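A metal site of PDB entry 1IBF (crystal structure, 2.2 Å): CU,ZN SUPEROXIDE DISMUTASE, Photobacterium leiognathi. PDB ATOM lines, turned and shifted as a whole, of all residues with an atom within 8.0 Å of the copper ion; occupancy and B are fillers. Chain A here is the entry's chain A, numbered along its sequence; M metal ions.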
ATOM      1  N   GLY A  43      16.157 -21.312 -13.546  1.00  0.00           N
ATOM      2  CA  GLY A  43      15.906 -20.021 -12.946  1.00  0.00           C
ATOM      3  C   GLY A  43      14.780 -20.220 -11.948  1.00  0.00           C
ATOM      4  O   GLY A  43      13.784 -20.865 -12.267  1.00  0.00           O
ATOM      5  N   PHE A  44      14.934 -19.671 -10.750  1.00  0.00           N
ATOM      6  CA  PHE A  44      13.956 -19.854  -9.682  1.00  0.00           C
ATOM      7  C   PHE A  44      13.685 -18.522  -8.988  1.00  0.00           C
ATOM      8  O   PHE A  44      14.551 -18.017  -8.275  1.00  0.00           O
ATOM      9  CB  PHE A  44      14.507 -20.811  -8.661  1.00  0.00           C
ATOM     10  CG  PHE A  44      13.547 -21.379  -7.659  1.00  0.00           C
ATOM     11  CD1 PHE A  44      12.255 -21.745  -8.000  1.00  0.00           C
ATOM     12  CD2 PHE A  44      14.008 -21.592  -6.372  1.00  0.00           C
ATOM     13  CE1 PHE A  44      11.420 -22.343  -7.063  1.00  0.00           C
ATOM     14  CE2 PHE A  44      13.173 -22.183  -5.428  1.00  0.00           C
ATOM     15  CZ  PHE A  44      11.888 -22.549  -5.781  1.00  0.00           C
ATOM     16  N   HIS A  45      12.495 -17.933  -9.165  1.00  0.00           N
ATOM     17  CA  HIS A  45      12.186 -16.643  -8.558  1.00  0.00           C
ATOM     18  C   HIS A  45      10.756 -16.519  -8.092  1.00  0.00           C
ATOM     19  O   HIS A  45       9.879 -17.247  -8.538  1.00  0.00           O
ATOM     20  CB  HIS A  45      12.450 -15.491  -9.530  1.00  0.00           C
ATOM     21  CG  HIS A  45      13.525 -15.843 -10.594  1.00  0.00           C
ATOM     22  ND1 HIS A  45      13.239 -16.113 -11.912  1.00  0.00           N
ATOM     23  CD2 HIS A  45      14.868 -15.941 -10.472  1.00  0.00           C
ATOM     24  CE1 HIS A  45      14.358 -16.368 -12.566  1.00  0.00           C
ATOM     25  NE2 HIS A  45      15.368 -16.269 -11.716  1.00  0.00           N
ATOM     26  N   ILE A  46      10.535 -15.591  -7.167  1.00  0.00           N
ATOM     27  CA  ILE A  46       9.173 -15.343  -6.720  1.00  0.00           C
ATOM     28  C   ILE A  46       8.709 -14.240  -7.684  1.00  0.00           C
ATOM     29  O   ILE A  46       9.489 -13.340  -8.001  1.00  0.00           O
ATOM     30  CB  ILE A  46       9.089 -14.764  -5.287  1.00  0.00           C
ATOM     31  CG1 ILE A  46       9.625 -15.767  -4.241  1.00  0.00           C
ATOM     32  CG2 ILE A  46       7.640 -14.362  -5.007  1.00  0.00           C
ATOM     33  CD1 ILE A  46       8.940 -17.141  -4.249  1.00  0.00           C
ATOM     34  N   HIS A  47       7.474 -14.304  -8.142  1.00  0.00           N
ATOM     35  CA  HIS A  47       6.959 -13.294  -9.085  1.00  0.00           C
ATOM     36  C   HIS A  47       5.906 -12.401  -8.465  1.00  0.00           C
ATOM     37  O   HIS A  47       5.294 -12.749  -7.452  1.00  0.00           O
ATOM     38  CB  HIS A  47       6.363 -13.952 -10.335  1.00  0.00           C
ATOM     39  CG  HIS A  47       7.434 -14.177 -11.402  1.00  0.00           C
ATOM     40  ND1 HIS A  47       7.486 -13.503 -12.599  1.00  0.00           N
ATOM     41  CD2 HIS A  47       8.507 -15.001 -11.380  1.00  0.00           C
ATOM     42  CE1 HIS A  47       8.554 -13.896 -13.273  1.00  0.00           C
ATOM     43  NE2 HIS A  47       9.191 -14.810 -12.555  1.00  0.00           N
ATOM     44  N   ALA A  67       1.824 -13.892 -14.246  1.00  0.00           N
ATOM     45  CA  ALA A  67       2.512 -13.734 -12.970  1.00  0.00           C
ATOM     46  C   ALA A  67       3.263 -12.417 -12.907  1.00  0.00           C
ATOM     47  O   ALA A  67       3.606 -11.944 -11.820  1.00  0.00           O
ATOM     48  CB  ALA A  67       3.469 -14.896 -12.742  1.00  0.00           C
ATOM     49  N   GLY A  68       3.510 -11.811 -14.064  1.00  0.00           N
ATOM     50  CA  GLY A  68       4.231 -10.542 -14.108  1.00  0.00           C
ATOM     51  C   GLY A  68       5.733 -10.758 -13.974  1.00  0.00           C
ATOM     52  O   GLY A  68       6.237 -11.860 -14.190  1.00  0.00           O
ATOM     53  N   GLY A  69       6.447  -9.681 -13.619  1.00  0.00           N
ATOM     54  CA  GLY A  69       7.887  -9.768 -13.456  1.00  0.00           C
ATOM     55  C   GLY A  69       8.303 -10.314 -12.102  1.00  0.00           C
ATOM     56  O   GLY A  69       7.468 -10.757 -11.323  1.00  0.00           O
ATOM     57  N   HIS A  70       9.605 -10.274 -11.825  1.00  0.00           N
ATOM     58  CA  HIS A  70      10.162 -10.757 -10.561  1.00  0.00           C
ATOM     59  C   HIS A  70       9.702  -9.904  -9.390  1.00  0.00           C
ATOM     60  O   HIS A  70       9.573  -8.685  -9.504  1.00  0.00           O
ATOM     61  CB  HIS A  70      11.707 -10.730 -10.601  1.00  0.00           C
ATOM     62  CG  HIS A  70      12.322 -11.668 -11.590  1.00  0.00           C
ATOM     63  ND1 HIS A  70      13.679 -11.872 -11.680  1.00  0.00           N
ATOM     64  CD2 HIS A  70      11.767 -12.461 -12.536  1.00  0.00           C
ATOM     65  CE1 HIS A  70      13.941 -12.738 -12.639  1.00  0.00           C
ATOM     66  NE2 HIS A  70      12.793 -13.120 -13.173  1.00  0.00           N
ATOM     67  N   TYR A  71       9.453 -10.552  -8.251  1.00  0.00           N
ATOM     68  CA  TYR A  71       9.026  -9.827  -7.059  1.00  0.00           C
ATOM     69  C   TYR A  71      10.115  -8.781  -6.779  1.00  0.00           C
ATOM     70  O   TYR A  71      11.291  -9.120  -6.670  1.00  0.00           O
ATOM     71  CB  TYR A  71       8.896 -10.813  -5.895  1.00  0.00           C
ATOM     72  CG  TYR A  71       8.492 -10.201  -4.566  1.00  0.00           C
ATOM     73  CD1 TYR A  71       7.449  -9.280  -4.482  1.00  0.00           C
ATOM     74  CD2 TYR A  71       9.128 -10.593  -3.396  1.00  0.00           C
ATOM     75  CE1 TYR A  71       7.045  -8.771  -3.249  1.00  0.00           C
ATOM     76  CE2 TYR A  71       8.733 -10.094  -2.167  1.00  0.00           C
ATOM     77  CZ  TYR A  71       7.697  -9.174  -2.094  1.00  0.00           C
ATOM     78  OH  TYR A  71       7.319  -8.701  -0.855  1.00  0.00           O
ATOM     79  N   HIS A  79      18.219  -7.396 -11.669  1.00  0.00           N
ATOM     80  CA  HIS A  79      18.203  -8.799 -11.310  1.00  0.00           C
ATOM     81  C   HIS A  79      19.581  -9.143 -10.739  1.00  0.00           C
ATOM     82  O   HIS A  79      20.605  -8.814 -11.333  1.00  0.00           O
ATOM     83  CB  HIS A  79      17.883  -9.639 -12.544  1.00  0.00           C
ATOM     84  CG  HIS A  79      17.905 -11.112 -12.293  1.00  0.00           C
ATOM     85  ND1 HIS A  79      16.891 -11.764 -11.608  1.00  0.00           N
ATOM     86  CD2 HIS A  79      18.842 -12.047 -12.561  1.00  0.00           C
ATOM     87  CE1 HIS A  79      17.207 -13.042 -11.474  1.00  0.00           C
ATOM     88  NE2 HIS A  79      18.390 -13.240 -12.050  1.00  0.00           N
ATOM     89  N   GLY A  90      12.815 -10.945  -4.998  1.00  0.00           N
ATOM     90  CA  GLY A  90      12.278 -12.258  -5.329  1.00  0.00           C
ATOM     91  C   GLY A  90      13.275 -13.219  -5.964  1.00  0.00           C
ATOM     92  O   GLY A  90      12.919 -14.349  -6.298  1.00  0.00           O
ATOM     93  N   ASP A  91      14.509 -12.750  -6.125  1.00  0.00           N
ATOM     94  CA  ASP A  91      15.558 -13.571  -6.715  1.00  0.00           C
ATOM     95  C   ASP A  91      16.015 -14.668  -5.731  1.00  0.00           C
ATOM     96  O   ASP A  91      16.529 -14.394  -4.640  1.00  0.00           O
ATOM     97  CB  ASP A  91      16.754 -12.685  -7.116  1.00  0.00           C
ATOM     98  CG  ASP A  91      16.399 -11.703  -8.227  1.00  0.00           C
ATOM     99  OD1 ASP A  91      15.459 -11.990  -9.002  1.00  0.00           O
ATOM    100  OD2 ASP A  91      17.059 -10.661  -8.337  1.00  0.00           O
ATOM    101  N   ALA A 121       3.429 -15.731  -6.851  1.00  0.00           N
ATOM    102  CA  ALA A 121       3.672 -16.959  -7.572  1.00  0.00           C
ATOM    103  C   ALA A 121       5.144 -17.323  -7.551  1.00  0.00           C
ATOM    104  O   ALA A 121       6.022 -16.457  -7.499  1.00  0.00           O
ATOM    105  CB  ALA A 121       3.197 -16.811  -9.029  1.00  0.00           C
ATOM    106  N   ILE A 122       5.405 -18.623  -7.564  1.00  0.00           N
ATOM    107  CA  ILE A 122       6.757 -19.150  -7.604  1.00  0.00           C
ATOM    108  C   ILE A 122       6.878 -19.677  -9.026  1.00  0.00           C
ATOM    109  O   ILE A 122       6.016 -20.411  -9.504  1.00  0.00           O
ATOM    110  CB  ILE A 122       6.967 -20.323  -6.624  1.00  0.00           C
ATOM    111  CG1 ILE A 122       6.581 -19.934  -5.208  1.00  0.00           C
ATOM    112  CG2 ILE A 122       8.437 -20.722  -6.654  1.00  0.00           C
ATOM    113  CD1 ILE A 122       6.662 -21.101  -4.222  1.00  0.00           C
ATOM    114  N   MET A 123       7.965 -19.298  -9.681  1.00  0.00           N
ATOM    115  CA  MET A 123       8.212 -19.657 -11.072  1.00  0.00           C
ATOM    116  C   MET A 123       9.515 -20.443 -11.228  1.00  0.00           C
ATOM    117  O   MET A 123      10.493 -20.180 -10.520  1.00  0.00           O
ATOM    118  CB  MET A 123       8.314 -18.362 -11.896  1.00  0.00           C
ATOM    119  CG  MET A 123       8.107 -18.490 -13.391  1.00  0.00           C
ATOM    120  SD  MET A 123       6.406 -18.943 -13.731  1.00  0.00           S
ATOM    121  CE  MET A 123       5.512 -17.356 -13.510  1.00  0.00           C
ATOM    122  N   ILE A 124       9.506 -21.413 -12.130  1.00  0.00           N
ATOM    123  CA  ILE A 124      10.702 -22.205 -12.438  1.00  0.00           C
ATOM    124  C   ILE A 124      10.867 -21.988 -13.933  1.00  0.00           C
ATOM    125  O   ILE A 124       9.913 -22.123 -14.693  1.00  0.00           O
ATOM    126  CB  ILE A 124      10.498 -23.700 -12.155  1.00  0.00           C
ATOM    127  CG1 ILE A 124      10.282 -23.912 -10.657  1.00  0.00           C
ATOM    128  CG2 ILE A 124      11.721 -24.484 -12.676  1.00  0.00           C
ATOM    129  CD1 ILE A 124       9.993 -25.350 -10.261  1.00  0.00           C
ATOM    130  N   HIS A 125      12.070 -21.612 -14.348  1.00  0.00           N
ATOM    131  CA  HIS A 125      12.357 -21.340 -15.756  1.00  0.00           C
ATOM    132  C   HIS A 125      13.086 -22.474 -16.448  1.00  0.00           C
ATOM    133  O   HIS A 125      13.588 -23.395 -15.792  1.00  0.00           O
ATOM    134  CB  HIS A 125      13.192 -20.069 -15.881  1.00  0.00           C
ATOM    135  CG  HIS A 125      12.462 -18.829 -15.479  1.00  0.00           C
ATOM    136  ND1 HIS A 125      12.087 -17.858 -16.372  1.00  0.00           N
ATOM    137  CD2 HIS A 125      11.976 -18.450 -14.276  1.00  0.00           C
ATOM    138  CE1 HIS A 125      11.394 -16.930 -15.739  1.00  0.00           C
ATOM    139  NE2 HIS A 125      11.309 -17.262 -14.467  1.00  0.00           N
ATOM    140  N   ASP A 129      20.339 -19.268 -14.200  1.00  0.00           N
ATOM    141  CA  ASP A 129      20.298 -17.952 -13.584  1.00  0.00           C
ATOM    142  C   ASP A 129      21.694 -17.561 -13.134  1.00  0.00           C
ATOM    143  O   ASP A 129      22.191 -18.082 -12.133  1.00  0.00           O
ATOM    144  CB  ASP A 129      19.355 -17.982 -12.365  1.00  0.00           C
ATOM    145  CG  ASP A 129      19.085 -16.603 -11.802  1.00  0.00           C
ATOM    146  OD1 ASP A 129      19.836 -15.653 -12.111  1.00  0.00           O
ATOM    147  OD2 ASP A 129      18.112 -16.479 -11.020  1.00  0.00           O
ATOM    148  N   LEU A 138      17.311 -10.879 -16.851  1.00  0.00           N
ATOM    149  CA  LEU A 138      16.734 -11.737 -15.835  1.00  0.00           C
ATOM    150  C   LEU A 138      17.535 -13.014 -15.540  1.00  0.00           C
ATOM    151  O   LEU A 138      16.994 -13.977 -15.010  1.00  0.00           O
ATOM    152  CB  LEU A 138      15.310 -12.083 -16.260  1.00  0.00           C
ATOM    153  CG  LEU A 138      14.549 -10.840 -16.719  1.00  0.00           C
ATOM    154  CD1 LEU A 138      13.151 -11.214 -17.171  1.00  0.00           C
ATOM    155  CD2 LEU A 138      14.483  -9.844 -15.557  1.00  0.00           C
ATOM    156  N   GLY A 141      17.007 -16.960 -17.547  1.00  0.00           N
ATOM    157  CA  GLY A 141      16.038 -17.990 -17.208  1.00  0.00           C
ATOM    158  C   GLY A 141      15.178 -18.392 -18.402  1.00  0.00           C
ATOM    159  O   GLY A 141      14.792 -19.561 -18.548  1.00  0.00           O
ATOM    160  N   GLY A 142      14.867 -17.414 -19.242  1.00  0.00           N
ATOM    161  CA  GLY A 142      14.080 -17.677 -20.427  1.00  0.00           C
ATOM    162  C   GLY A 142      12.609 -17.976 -20.160  1.00  0.00           C
ATOM    163  O   GLY A 142      12.017 -17.406 -19.251  1.00  0.00           O
ATOM    164  N   ALA A 143      12.024 -18.865 -20.949  1.00  0.00           N
ATOM    165  CA  ALA A 143      10.625 -19.216 -20.788  1.00  0.00           C
ATOM    166  C   ALA A 143      10.358 -19.784 -19.390  1.00  0.00           C
ATOM    167  O   ALA A 143      11.259 -20.286 -18.727  1.00  0.00           O
ATOM    168  CB  ALA A 143      10.206 -20.219 -21.856  1.00  0.00           C
ATOM    169  N   ARG A 144       9.104 -19.693 -18.968  1.00  0.00           N
ATOM    170  CA  ARG A 144       8.678 -20.193 -17.672  1.00  0.00           C
ATOM    171  C   ARG A 144       8.147 -21.606 -17.891  1.00  0.00           C
ATOM    172  O   ARG A 144       7.224 -21.810 -18.682  1.00  0.00           O
ATOM    173  CB  ARG A 144       7.585 -19.265 -17.125  1.00  0.00           C
ATOM    174  CG  ARG A 144       7.980 -17.810 -17.247  1.00  0.00           C
ATOM    175  CD  ARG A 144       6.915 -16.834 -16.791  1.00  0.00           C
ATOM    176  NE  ARG A 144       7.459 -15.470 -16.858  1.00  0.00           N
ATOM    177  CZ  ARG A 144       6.889 -14.399 -16.319  1.00  0.00           C
ATOM    178  NH1 ARG A 144       5.754 -14.495 -15.646  1.00  0.00           N
ATOM    179  NH2 ARG A 144       7.480 -13.221 -16.446  1.00  0.00           N
ATOM    180  N   ALA A 146       7.471 -24.061 -15.138  1.00  0.00           N
ATOM    181  CA  ALA A 146       6.635 -24.544 -14.048  1.00  0.00           C
ATOM    182  C   ALA A 146       6.204 -23.390 -13.143  1.00  0.00           C
ATOM    183  O   ALA A 146       6.989 -22.471 -12.883  1.00  0.00           O
ATOM    184  CB  ALA A 146       7.392 -25.596 -13.226  1.00  0.00           C
HETATM  185 CU    CU M   1      11.198 -15.986 -12.745  1.00  0.00          CU
HETATM  186 ZN    ZN M   2      15.194 -11.052 -10.592  1.00  0.00          ZN
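The backbone NH (N) of His 125 sits at hydrogen-bond distance from the backbone carbonyl oxygen (O) of Gly 43.
N of Met 123 lies within hydrogen-bond range of O of His 45, 3.0 Å away.
A ring nitrogen (ND1) of His 125 lies close to the backbone carbonyl oxygen of Ala 143, at 3.5 Å.
ND1 of His 47 is in hydrogen-bond range of O of Gly 68 (2.6 Å).
N of His 47 sits at hydrogen-bond distance from O of Ala 121 (2.7 Å).
A ring nitrogen (ND1) of His 125 is in hydrogen-bond range of the backbone carbonyl oxygen (O) of Gly 142 (2.9 Å).
The backbone carbonyl oxygen of Gly 69 is in hydrogen-bond range of a ring nitrogen (ND1) of His 47 (3.0 Å).
ND1 of His 45 sits close to NE2 of His 70 (3.3 Å).
Residues that only touch the copper ion: His 70 (3.3 Å) and Met 123 (3.8 Å).
Five residues have an atom within 4 Å of the copper ion: His 45, His 47, His 70, Met 123 and His 125.
The nearest printed residue that does not touch the copper ion is Phe 44 (5.2 Å).
The copper ion is bound by a ring nitrogen (NE2) of His 125 (2.1 Å), a ring nitrogen (ND1) of His 45 (2.2 Å) and a ring nitrogen (NE2) of His 47 (2.3 Å).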
